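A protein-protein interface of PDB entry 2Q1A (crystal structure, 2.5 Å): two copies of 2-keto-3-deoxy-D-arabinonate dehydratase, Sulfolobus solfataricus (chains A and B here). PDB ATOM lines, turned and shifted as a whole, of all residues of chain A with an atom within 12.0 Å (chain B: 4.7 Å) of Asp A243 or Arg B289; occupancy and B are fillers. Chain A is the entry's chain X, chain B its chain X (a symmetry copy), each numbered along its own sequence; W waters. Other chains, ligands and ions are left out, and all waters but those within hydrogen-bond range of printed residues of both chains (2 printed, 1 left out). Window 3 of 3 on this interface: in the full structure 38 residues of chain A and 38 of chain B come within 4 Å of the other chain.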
ATOM      1  N   GLU A  75      19.832   0.465   5.841  1.00  0.00           N
ATOM      2  CA  GLU A  75      21.057   0.982   6.446  1.00  0.00           C
ATOM      3  C   GLU A  75      21.279   0.324   7.813  1.00  0.00           C
ATOM      4  O   GLU A  75      20.317  -0.047   8.494  1.00  0.00           O
ATOM      5  CB  GLU A  75      20.979   2.507   6.612  1.00  0.00           C
ATOM      6  CG  GLU A  75      20.572   3.279   5.354  1.00  0.00           C
ATOM      7  CD  GLU A  75      20.681   4.793   5.504  1.00  0.00           C
ATOM      8  OE1 GLU A  75      20.819   5.298   6.642  1.00  0.00           O
ATOM      9  OE2 GLU A  75      20.629   5.483   4.467  1.00  0.00           O
ATOM     10  N   TRP A  77      23.586   1.225  11.359  1.00  0.00           N
ATOM     11  CA  TRP A  77      24.478   2.141  12.066  1.00  0.00           C
ATOM     12  C   TRP A  77      24.876   1.584  13.425  1.00  0.00           C
ATOM     13  O   TRP A  77      24.114   0.846  14.064  1.00  0.00           O
ATOM     14  CB  TRP A  77      23.833   3.514  12.269  1.00  0.00           C
ATOM     15  CG  TRP A  77      23.531   4.289  11.020  1.00  0.00           C
ATOM     16  CD1 TRP A  77      22.550   4.028  10.112  1.00  0.00           C
ATOM     17  CD2 TRP A  77      24.179   5.489  10.574  1.00  0.00           C
ATOM     18  NE1 TRP A  77      22.553   4.976   9.119  1.00  0.00           N
ATOM     19  CE2 TRP A  77      23.539   5.889   9.379  1.00  0.00           C
ATOM     20  CE3 TRP A  77      25.237   6.267  11.068  1.00  0.00           C
ATOM     21  CZ2 TRP A  77      23.928   7.024   8.661  1.00  0.00           C
ATOM     22  CZ3 TRP A  77      25.623   7.398  10.351  1.00  0.00           C
ATOM     23  CH2 TRP A  77      24.965   7.764   9.164  1.00  0.00           C
ATOM     24  N   ARG A 112      27.943  14.360  23.469  1.00  0.00           N
ATOM     25  CA  ARG A 112      27.745  13.714  22.175  1.00  0.00           C
ATOM     26  C   ARG A 112      28.338  12.293  22.163  1.00  0.00           C
ATOM     27  O   ARG A 112      29.546  12.119  22.361  1.00  0.00           O
ATOM     28  CB  ARG A 112      28.370  14.564  21.062  1.00  0.00           C
ATOM     29  CG  ARG A 112      28.096  14.061  19.647  1.00  0.00           C
ATOM     30  CD  ARG A 112      28.818  14.900  18.588  1.00  0.00           C
ATOM     31  NE  ARG A 112      28.307  16.271  18.514  1.00  0.00           N
ATOM     32  CZ  ARG A 112      27.252  16.661  17.796  1.00  0.00           C
ATOM     33  NH1 ARG A 112      26.886  17.935  17.810  1.00  0.00           N
ATOM     34  NH2 ARG A 112      26.564  15.796  17.062  1.00  0.00           N
ATOM     35  N   ILE A 115      28.644   7.719  16.990  1.00  0.00           N
ATOM     36  CA  ILE A 115      27.751   7.099  16.020  1.00  0.00           C
ATOM     37  C   ILE A 115      28.535   6.977  14.715  1.00  0.00           C
ATOM     38  O   ILE A 115      29.149   7.951  14.263  1.00  0.00           O
ATOM     39  CB  ILE A 115      26.479   7.968  15.772  1.00  0.00           C
ATOM     40  CG1 ILE A 115      25.738   8.287  17.082  1.00  0.00           C
ATOM     41  CG2 ILE A 115      25.553   7.338  14.717  1.00  0.00           C
ATOM     42  CD1 ILE A 115      24.883   7.168  17.650  1.00  0.00           C
ATOM     43  N   SER A 152      11.271   5.565  10.292  1.00  0.00           N
ATOM     44  CA  SER A 152      11.898   6.822   9.854  1.00  0.00           C
ATOM     45  C   SER A 152      11.865   7.950  10.889  1.00  0.00           C
ATOM     46  O   SER A 152      12.636   8.904  10.785  1.00  0.00           O
ATOM     47  CB  SER A 152      11.338   7.294   8.504  1.00  0.00           C
ATOM     48  OG  SER A 152       9.920   7.288   8.490  1.00  0.00           O
ATOM     49  N   ASN A 153      10.998   7.830  11.892  1.00  0.00           N
ATOM     50  CA  ASN A 153      10.944   8.805  12.984  1.00  0.00           C
ATOM     51  C   ASN A 153      11.830   8.442  14.164  1.00  0.00           C
ATOM     52  O   ASN A 153      11.972   9.226  15.105  1.00  0.00           O
ATOM     53  CB  ASN A 153       9.506   9.004  13.474  1.00  0.00           C
ATOM     54  CG  ASN A 153       8.571   9.473  12.378  1.00  0.00           C
ATOM     55  OD1 ASN A 153       7.465   8.961  12.248  1.00  0.00           O
ATOM     56  ND2 ASN A 153       9.014  10.443  11.578  1.00  0.00           N
ATOM     57  N   GLY A 154      12.420   7.253  14.124  1.00  0.00           N
ATOM     58  CA  GLY A 154      13.312   6.805  15.194  1.00  0.00           C
ATOM     59  C   GLY A 154      12.600   6.012  16.268  1.00  0.00           C
ATOM     60  O   GLY A 154      13.114   5.854  17.372  1.00  0.00           O
ATOM     61  N   GLU A 235      18.928   8.145  23.474  1.00  0.00           N
ATOM     62  CA  GLU A 235      19.891   9.215  23.218  1.00  0.00           C
ATOM     63  C   GLU A 235      20.723   8.900  21.975  1.00  0.00           C
ATOM     64  O   GLU A 235      21.079   9.803  21.207  1.00  0.00           O
ATOM     65  CB  GLU A 235      20.793   9.416  24.438  1.00  0.00           C
ATOM     66  CG  GLU A 235      21.666  10.673  24.411  1.00  0.00           C
ATOM     67  CD  GLU A 235      22.486  10.844  25.692  1.00  0.00           C
ATOM     68  OE1 GLU A 235      21.883  10.896  26.788  1.00  0.00           O
ATOM     69  OE2 GLU A 235      23.732  10.926  25.606  1.00  0.00           O
ATOM     70  N   GLN A 236      21.023   7.615  21.792  1.00  0.00           N
ATOM     71  CA  GLN A 236      21.742   7.135  20.617  1.00  0.00           C
ATOM     72  C   GLN A 236      20.895   7.367  19.365  1.00  0.00           C
ATOM     73  O   GLN A 236      21.401   7.847  18.347  1.00  0.00           O
ATOM     74  CB  GLN A 236      22.078   5.647  20.759  1.00  0.00           C
ATOM     75  CG  GLN A 236      22.997   5.295  21.926  1.00  0.00           C
ATOM     76  CD  GLN A 236      23.217   3.789  22.074  1.00  0.00           C
ATOM     77  OE1 GLN A 236      23.386   3.070  21.090  1.00  0.00           O
ATOM     78  NE2 GLN A 236      23.217   3.314  23.312  1.00  0.00           N
ATOM     79  N   ILE A 237      19.608   7.033  19.460  1.00  0.00           N
ATOM     80  CA  ILE A 237      18.647   7.273  18.389  1.00  0.00           C
ATOM     81  C   ILE A 237      18.573   8.763  18.064  1.00  0.00           C
ATOM     82  O   ILE A 237      18.610   9.152  16.898  1.00  0.00           O
ATOM     83  CB  ILE A 237      17.239   6.764  18.765  1.00  0.00           C
ATOM     84  CG1 ILE A 237      17.240   5.236  18.891  1.00  0.00           C
ATOM     85  CG2 ILE A 237      16.199   7.241  17.739  1.00  0.00           C
ATOM     86  CD1 ILE A 237      15.981   4.653  19.519  1.00  0.00           C
ATOM     87  N   GLN A 238      18.486   9.579  19.110  1.00  0.00           N
ATOM     88  CA  GLN A 238      18.389  11.031  18.992  1.00  0.00           C
ATOM     89  C   GLN A 238      19.510  11.611  18.128  1.00  0.00           C
ATOM     90  O   GLN A 238      19.252  12.423  17.238  1.00  0.00           O
ATOM     91  CB  GLN A 238      18.392  11.668  20.387  1.00  0.00           C
ATOM     92  CG  GLN A 238      18.165  13.185  20.420  1.00  0.00           C
ATOM     93  CD  GLN A 238      18.500  13.832  21.773  1.00  0.00           C
ATOM     94  OE1 GLN A 238      18.275  15.025  21.963  1.00  0.00           O
ATOM     95  NE2 GLN A 238      19.043  13.050  22.709  1.00  0.00           N
ATOM     96  N   TYR A 239      20.743  11.185  18.381  1.00  0.00           N
ATOM     97  CA  TYR A 239      21.893  11.732  17.670  1.00  0.00           C
ATOM     98  C   TYR A 239      22.032  11.170  16.255  1.00  0.00           C
ATOM     99  O   TYR A 239      22.538  11.856  15.352  1.00  0.00           O
ATOM    100  CB  TYR A 239      23.182  11.541  18.484  1.00  0.00           C
ATOM    101  CG  TYR A 239      23.390  12.627  19.521  1.00  0.00           C
ATOM    102  CD1 TYR A 239      22.702  12.601  20.736  1.00  0.00           C
ATOM    103  CD2 TYR A 239      24.256  13.696  19.276  1.00  0.00           C
ATOM    104  CE1 TYR A 239      22.875  13.606  21.685  1.00  0.00           C
ATOM    105  CE2 TYR A 239      24.437  14.705  20.217  1.00  0.00           C
ATOM    106  CZ  TYR A 239      23.744  14.652  21.421  1.00  0.00           C
ATOM    107  OH  TYR A 239      23.918  15.644  22.362  1.00  0.00           O
ATOM    108  N   LEU A 240      21.565   9.936  16.068  1.00  0.00           N
ATOM    109  CA  LEU A 240      21.598   9.277  14.767  1.00  0.00           C
ATOM    110  C   LEU A 240      20.708   9.980  13.732  1.00  0.00           C
ATOM    111  O   LEU A 240      21.118  10.164  12.587  1.00  0.00           O
ATOM    112  CB  LEU A 240      21.194   7.804  14.905  1.00  0.00           C
ATOM    113  CG  LEU A 240      20.863   7.049  13.609  1.00  0.00           C
ATOM    114  CD1 LEU A 240      22.128   6.769  12.832  1.00  0.00           C
ATOM    115  CD2 LEU A 240      20.079   5.772  13.881  1.00  0.00           C
ATOM    116  N   ILE A 241      19.499  10.362  14.145  1.00  0.00           N
ATOM    117  CA  ILE A 241      18.498  10.930  13.231  1.00  0.00           C
ATOM    118  C   ILE A 241      18.582  12.455  13.053  1.00  0.00           C
ATOM    119  O   ILE A 241      17.965  12.996  12.138  1.00  0.00           O
ATOM    120  CB  ILE A 241      17.038  10.508  13.601  1.00  0.00           C
ATOM    121  CG1 ILE A 241      16.639  11.018  14.993  1.00  0.00           C
ATOM    122  CG2 ILE A 241      16.876   8.994  13.504  1.00  0.00           C
ATOM    123  CD1 ILE A 241      15.148  10.878  15.314  1.00  0.00           C
ATOM    124  N   ARG A 242      19.343  13.131  13.916  1.00  0.00           N
ATOM    125  CA  ARG A 242      19.523  14.585  13.831  1.00  0.00           C
ATOM    126  C   ARG A 242      20.080  15.014  12.476  1.00  0.00           C
ATOM    127  O   ARG A 242      21.215  14.661  12.130  1.00  0.00           O
ATOM    128  CB  ARG A 242      20.448  15.082  14.943  1.00  0.00           C
ATOM    129  CG  ARG A 242      20.698  16.584  14.908  1.00  0.00           C
ATOM    130  CD  ARG A 242      21.550  17.034  16.080  1.00  0.00           C
ATOM    131  NE  ARG A 242      20.841  16.881  17.350  1.00  0.00           N
ATOM    132  CZ  ARG A 242      21.355  17.174  18.543  1.00  0.00           C
ATOM    133  NH1 ARG A 242      22.597  17.641  18.652  1.00  0.00           N
ATOM    134  NH2 ARG A 242      20.622  16.993  19.632  1.00  0.00           N
ATOM    135  N   ASP A 243      19.276  15.773  11.726  1.00  0.00           N
ATOM    136  CA  ASP A 243      19.626  16.221  10.371  1.00  0.00           C
ATOM    137  C   ASP A 243      19.976  15.075   9.418  1.00  0.00           C
ATOM    138  O   ASP A 243      20.699  15.259   8.439  1.00  0.00           O
ATOM    139  CB  ASP A 243      20.778  17.231  10.420  1.00  0.00           C
ATOM    140  CG  ASP A 243      20.421  18.476  11.177  1.00  0.00           C
ATOM    141  OD1 ASP A 243      19.291  18.969  10.996  1.00  0.00           O
ATOM    142  OD2 ASP A 243      21.268  18.957  11.951  1.00  0.00           O
ATOM    143  N   ASN A 244      19.443  13.891   9.706  1.00  0.00           N
ATOM    144  CA  ASN A 244      19.884  12.676   9.044  1.00  0.00           C
ATOM    145  C   ASN A 244      18.735  11.694   8.881  1.00  0.00           C
ATOM    146  O   ASN A 244      18.436  10.917   9.790  1.00  0.00           O
ATOM    147  CB  ASN A 244      21.045  12.048   9.816  1.00  0.00           C
ATOM    148  CG  ASN A 244      21.768  10.985   9.027  1.00  0.00           C
ATOM    149  OD1 ASN A 244      21.875  11.063   7.804  1.00  0.00           O
ATOM    150  ND2 ASN A 244      22.285   9.982   9.728  1.00  0.00           N
ATOM    151  N   PRO A 245      18.071  11.741   7.716  1.00  0.00           N
ATOM    152  CA  PRO A 245      16.950  10.849   7.455  1.00  0.00           C
ATOM    153  C   PRO A 245      17.425   9.408   7.348  1.00  0.00           C
ATOM    154  O   PRO A 245      18.425   9.135   6.683  1.00  0.00           O
ATOM    155  CB  PRO A 245      16.415  11.336   6.098  1.00  0.00           C
ATOM    156  CG  PRO A 245      17.602  11.980   5.436  1.00  0.00           C
ATOM    157  CD  PRO A 245      18.354  12.630   6.573  1.00  0.00           C
ATOM    158  N   ILE A 246      16.709   8.514   8.020  1.00  0.00           N
ATOM    159  CA  ILE A 246      16.950   7.076   7.944  1.00  0.00           C
ATOM    160  C   ILE A 246      15.682   6.405   7.426  1.00  0.00           C
ATOM    161  O   ILE A 246      14.579   6.752   7.852  1.00  0.00           O
ATOM    162  CB  ILE A 246      17.377   6.471   9.317  1.00  0.00           C
ATOM    163  CG1 ILE A 246      16.352   6.799  10.416  1.00  0.00           C
ATOM    164  CG2 ILE A 246      18.782   6.961   9.705  1.00  0.00           C
ATOM    165  CD1 ILE A 246      16.419   5.900  11.628  1.00  0.00           C
ATOM    166  N   PRO A 247      15.823   5.471   6.471  1.00  0.00           N
ATOM    167  CA  PRO A 247      14.631   4.786   5.958  1.00  0.00           C
ATOM    168  C   PRO A 247      13.999   3.811   6.961  1.00  0.00           C
ATOM    169  O   PRO A 247      14.653   3.399   7.919  1.00  0.00           O
ATOM    170  CB  PRO A 247      15.148   4.054   4.714  1.00  0.00           C
ATOM    171  CG  PRO A 247      16.623   3.956   4.889  1.00  0.00           C
ATOM    172  CD  PRO A 247      17.067   5.035   5.807  1.00  0.00           C
ATOM    173  N   ALA B 132      23.936  21.609   2.721  1.00  0.00           N
ATOM    174  CA  ALA B 132      23.440  21.913   4.055  1.00  0.00           C
ATOM    175  C   ALA B 132      24.513  21.944   5.128  1.00  0.00           C
ATOM    176  O   ALA B 132      25.541  21.274   5.028  1.00  0.00           O
ATOM    177  CB  ALA B 132      22.310  20.967   4.443  1.00  0.00           C
ATOM    178  N   VAL B 133      24.250  22.765   6.139  1.00  0.00           N
ATOM    179  CA  VAL B 133      25.102  22.937   7.301  1.00  0.00           C
ATOM    180  C   VAL B 133      24.291  22.373   8.450  1.00  0.00           C
ATOM    181  O   VAL B 133      23.137  22.774   8.642  1.00  0.00           O
ATOM    182  CB  VAL B 133      25.411  24.448   7.554  1.00  0.00           C
ATOM    183  CG1 VAL B 133      26.127  24.661   8.879  1.00  0.00           C
ATOM    184  CG2 VAL B 133      26.228  25.026   6.414  1.00  0.00           C
ATOM    185  N   ARG B 134      24.879  21.437   9.197  1.00  0.00           N
ATOM    186  CA  ARG B 134      24.204  20.810  10.337  1.00  0.00           C
ATOM    187  C   ARG B 134      23.701  21.849  11.344  1.00  0.00           C
ATOM    188  O   ARG B 134      24.340  22.882  11.554  1.00  0.00           O
ATOM    189  CB  ARG B 134      25.142  19.822  11.039  1.00  0.00           C
ATOM    190  CG  ARG B 134      25.298  18.465  10.351  1.00  0.00           C
ATOM    191  CD  ARG B 134      26.189  17.538  11.194  1.00  0.00           C
ATOM    192  NE  ARG B 134      25.570  17.261  12.487  1.00  0.00           N
ATOM    193  CZ  ARG B 134      25.099  16.078  12.870  1.00  0.00           C
ATOM    194  NH1 ARG B 134      25.209  15.015  12.074  1.00  0.00           N
ATOM    195  NH2 ARG B 134      24.533  15.957  14.066  1.00  0.00           N
ATOM    196  N   SER B 135      22.561  21.560  11.965  1.00  0.00           N
ATOM    197  CA  SER B 135      21.961  22.454  12.951  1.00  0.00           C
ATOM    198  C   SER B 135      22.888  22.731  14.143  1.00  0.00           C
ATOM    199  O   SER B 135      22.873  23.830  14.714  1.00  0.00           O
ATOM    200  CB  SER B 135      20.632  21.880  13.446  1.00  0.00           C
ATOM    201  OG  SER B 135      20.850  20.892  14.440  1.00  0.00           O
ATOM    202  N   ASP B 136      23.688  21.727  14.504  1.00  0.00           N
ATOM    203  CA  ASP B 136      24.606  21.806  15.640  1.00  0.00           C
ATOM    204  C   ASP B 136      26.059  21.997  15.220  1.00  0.00           C
ATOM    205  O   ASP B 136      26.969  21.620  15.949  1.00  0.00           O
ATOM    206  CB  ASP B 136      24.475  20.560  16.530  1.00  0.00           C
ATOM    207  CG  ASP B 136      24.693  19.239  15.766  1.00  0.00           C
ATOM    208  OD1 ASP B 136      25.079  19.239  14.570  1.00  0.00           O
ATOM    209  OD2 ASP B 136      24.465  18.179  16.383  1.00  0.00           O
ATOM    210  N   TYR B 184      25.018  13.196   6.309  1.00  0.00           N
ATOM    211  CA  TYR B 184      23.733  13.801   6.661  1.00  0.00           C
ATOM    212  C   TYR B 184      23.054  14.339   5.399  1.00  0.00           C
ATOM    213  O   TYR B 184      23.669  14.380   4.326  1.00  0.00           O
ATOM    214  CB  TYR B 184      23.916  14.922   7.704  1.00  0.00           C
ATOM    215  CG  TYR B 184      24.841  16.054   7.287  1.00  0.00           C
ATOM    216  CD1 TYR B 184      24.327  17.223   6.720  1.00  0.00           C
ATOM    217  CD2 TYR B 184      26.224  15.972   7.484  1.00  0.00           C
ATOM    218  CE1 TYR B 184      25.163  18.281   6.341  1.00  0.00           C
ATOM    219  CE2 TYR B 184      27.074  17.027   7.110  1.00  0.00           C
ATOM    220  CZ  TYR B 184      26.529  18.179   6.533  1.00  0.00           C
ATOM    221  OH  TYR B 184      27.341  19.232   6.149  1.00  0.00           O
ATOM    222  N   ALA B 185      21.795  14.746   5.525  1.00  0.00           N
ATOM    223  CA  ALA B 185      21.056  15.318   4.392  1.00  0.00           C
ATOM    224  C   ALA B 185      21.753  16.556   3.822  1.00  0.00           C
ATOM    225  O   ALA B 185      21.908  17.569   4.504  1.00  0.00           O
ATOM    226  CB  ALA B 185      19.612  15.635   4.786  1.00  0.00           C
ATOM    227  N   LYS B 287      22.107  26.196   2.776  1.00  0.00           N
ATOM    228  CA  LYS B 287      20.960  26.281   3.663  1.00  0.00           C
ATOM    229  C   LYS B 287      21.314  25.711   5.050  1.00  0.00           C
ATOM    230  O   LYS B 287      21.740  24.560   5.177  1.00  0.00           O
ATOM    231  CB  LYS B 287      19.764  25.555   3.026  1.00  0.00           C
ATOM    232  CG  LYS B 287      18.669  25.078   3.986  1.00  0.00           C
ATOM    233  CD  LYS B 287      17.721  26.207   4.376  1.00  0.00           C
ATOM    234  CE  LYS B 287      16.779  25.787   5.499  1.00  0.00           C
ATOM    235  NZ  LYS B 287      15.926  26.933   5.928  1.00  0.00           N
ATOM    236  N   LYS B 288      21.149  26.538   6.081  1.00  0.00           N
ATOM    237  CA  LYS B 288      21.385  26.143   7.467  1.00  0.00           C
ATOM    238  C   LYS B 288      20.181  25.395   8.043  1.00  0.00           C
ATOM    239  O   LYS B 288      19.047  25.879   7.961  1.00  0.00           O
ATOM    240  CB  LYS B 288      21.699  27.380   8.317  1.00  0.00           C
ATOM    241  CG  LYS B 288      21.704  27.155   9.829  1.00  0.00           C
ATOM    242  CD  LYS B 288      23.049  26.642  10.334  1.00  0.00           C
ATOM    243  CE  LYS B 288      23.059  26.529  11.853  1.00  0.00           C
ATOM    244  NZ  LYS B 288      24.418  26.204  12.365  1.00  0.00           N
ATOM    245  N   ARG B 289      20.440  24.223   8.628  1.00  0.00           N
ATOM    246  CA  ARG B 289      19.399  23.408   9.266  1.00  0.00           C
ATOM    247  C   ARG B 289      18.930  24.001  10.605  1.00  0.00           C
ATOM    248  O   ARG B 289      19.731  24.515  11.388  1.00  0.00           O
ATOM    249  CB  ARG B 289      19.871  21.957   9.460  1.00  0.00           C
ATOM    250  CG  ARG B 289      20.076  21.145   8.175  1.00  0.00           C
ATOM    251  CD  ARG B 289      18.760  20.880   7.436  1.00  0.00           C
ATOM    252  NE  ARG B 289      18.908  19.879   6.376  1.00  0.00           N
ATOM    253  CZ  ARG B 289      18.260  19.907   5.211  1.00  0.00           C
ATOM    254  NH1 ARG B 289      18.465  18.948   4.318  1.00  0.00           N
ATOM    255  NH2 ARG B 289      17.419  20.896   4.926  1.00  0.00           N
ATOM    256  N   ARG B 290      17.625  23.911  10.849  1.00  0.00           N
ATOM    257  CA  ARG B 290      16.988  24.472  12.040  1.00  0.00           C
ATOM    258  C   ARG B 290      16.756  23.373  13.092  1.00  0.00           C
ATOM    259  O   ARG B 290      16.380  22.247  12.746  1.00  0.00           O
ATOM    260  CB  ARG B 290      15.672  25.154  11.639  1.00  0.00           C
ATOM    261  CG  ARG B 290      14.925  25.843  12.773  1.00  0.00           C
ATOM    262  CD  ARG B 290      13.561  26.389  12.324  1.00  0.00           C
ATOM    263  NE  ARG B 290      12.578  26.379  13.416  1.00  0.00           N
ATOM    264  CZ  ARG B 290      12.564  27.230  14.449  1.00  0.00           C
ATOM    265  NH1 ARG B 290      13.488  28.183  14.564  1.00  0.00           N
ATOM    266  NH2 ARG B 290      11.623  27.123  15.381  1.00  0.00           N
ATOM    267  N   LYS B 291      16.975  23.708  14.367  1.00  0.00           N
ATOM    268  CA  LYS B 291      16.954  22.725  15.469  1.00  0.00           C
ATOM    269  C   LYS B 291      15.591  22.072  15.739  1.00  0.00           C
ATOM    270  O   LYS B 291      14.593  22.752  15.970  1.00  0.00           O
ATOM    271  CB  LYS B 291      17.522  23.339  16.757  1.00  0.00           C
ATOM    272  CG  LYS B 291      19.026  23.588  16.697  1.00  0.00           C
ATOM    273  CD  LYS B 291      19.588  24.070  18.026  1.00  0.00           C
ATOM    274  CE  LYS B 291      21.106  24.211  17.945  1.00  0.00           C
ATOM    275  NZ  LYS B 291      21.692  24.816  19.180  1.00  0.00           N
HETATM  276  O   HOH W   1      20.602  18.008   7.053  1.00  0.00           O
HETATM  277  O   HOH W   2      24.194  13.907  15.465  1.00  0.00           O
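OD2 of Asp B136 lies within salt-bridge range of NH1 of Arg A242 (3.0 Å). N of Ser B135 sits at hydrogen-bond distance from OD2 of Asp A243, 2.9 Å away. The guanidinium group (NH1) of Arg A112 is in salt-bridge range of the side-chain carboxylate (OD2) of Asp B136, 2.8 Å away. O of Asp A243 sits at hydrogen-bond distance from N of Ala B185, 3.2 Å away.
No position is printed for both chains. Of the 11 pairs that touch across the chains among the printed residues, none has its exchanged pair printed and touching as well.
Water W2 lies within hydrogen-bond range of the guanidinium group of Arg B134, the backbone carbonyl oxygen of Tyr A239 and the guanidinium group of Arg A112. Water W1 lies within hydrogen-bond range of the guanidinium group (NE) of Arg B289 (2.6 Å), the backbone carbonyl oxygen (O) of Ala B185 (2.9 Å) and the backbone carbonyl oxygen (O) of Asp A243 (3.1 Å).
The backbone carbonyl oxygen (O) of Ala B132 sits at hydrogen-bond distance from the side-chain hydroxyl (OH) of Tyr B184 (2.9 Å). O of Arg B134 lies within hydrogen-bond range of NZ of Lys B288 (3.4 Å). O of Val B133 is in hydrogen-bond range of N of Arg B289, at 3.1 Å. NE of Arg B134 is in salt-bridge range of OD1 of Asp B136 (2.9 Å). O of Leu A240 sits at hydrogen-bond distance from ND2 of Asn A244 (3.1 Å).
Hydrophobic or aromatic side chains of chain B within 4 Å of the printed part of chain A: Tyr B184 and Ala B185. Along chain B the printed residues that touch a printed residue of chain A span positions 134 to 289. Printed residues of chain A that touch a printed residue of chain B: Arg A112, Arg A242, Asp A243, Asn A244 and Pro A245. Hydrophobic or aromatic side chains of chain A within 4 Å of the printed part of chain B: Pro A245.
Arg B134 touches Arg A112. Arg A242 touches Arg B134. OD2 of Asp A243 touches C of Arg B134 (3.8 Å). Asp A243 touches Tyr B184. Asp A243 touches Arg B289 (OD1 to CB, 3.4 Å). OD1 of Asn A244 touches CA of Tyr B184, at 3.5 Å. Pro A245 touches Ala B185 (CD to CB, 3.7 Å).
Of the printed residues of chain B, Asp A243 touches Arg B134, Ser B135, Tyr B184, Ala B185 and Arg B289. Of chain A, only Asp A243 (3.4 Å) comes within 4 Å of Arg B289. No residue of chain A comes within 4 Å of Ala B132. Ser B135 touches one residue of chain A. Of chain A, only Asp A243 and Pro A245 come within 4 Å of Ala B185. No residue of chain A comes within 4 Å of Lys B287. No residue of chain A comes within 4 Å of Lys B288. Printed residues of chain B within 4 Å of Arg A242: Arg B134 and Asp B136. Of the printed residues of chain B, Arg A112 touches Arg B134 and Asp B136. Of the printed residues of chain B, Asn A244 touches Tyr B184. Gln A238 touches none of the printed residues of chain B. The nearest residue of chain B that does not touch Asp A243 is Asp B136 (4.5 Å). The nearest printed residue of chain B that does not touch Pro A245 is Tyr B184 (5.1 Å).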
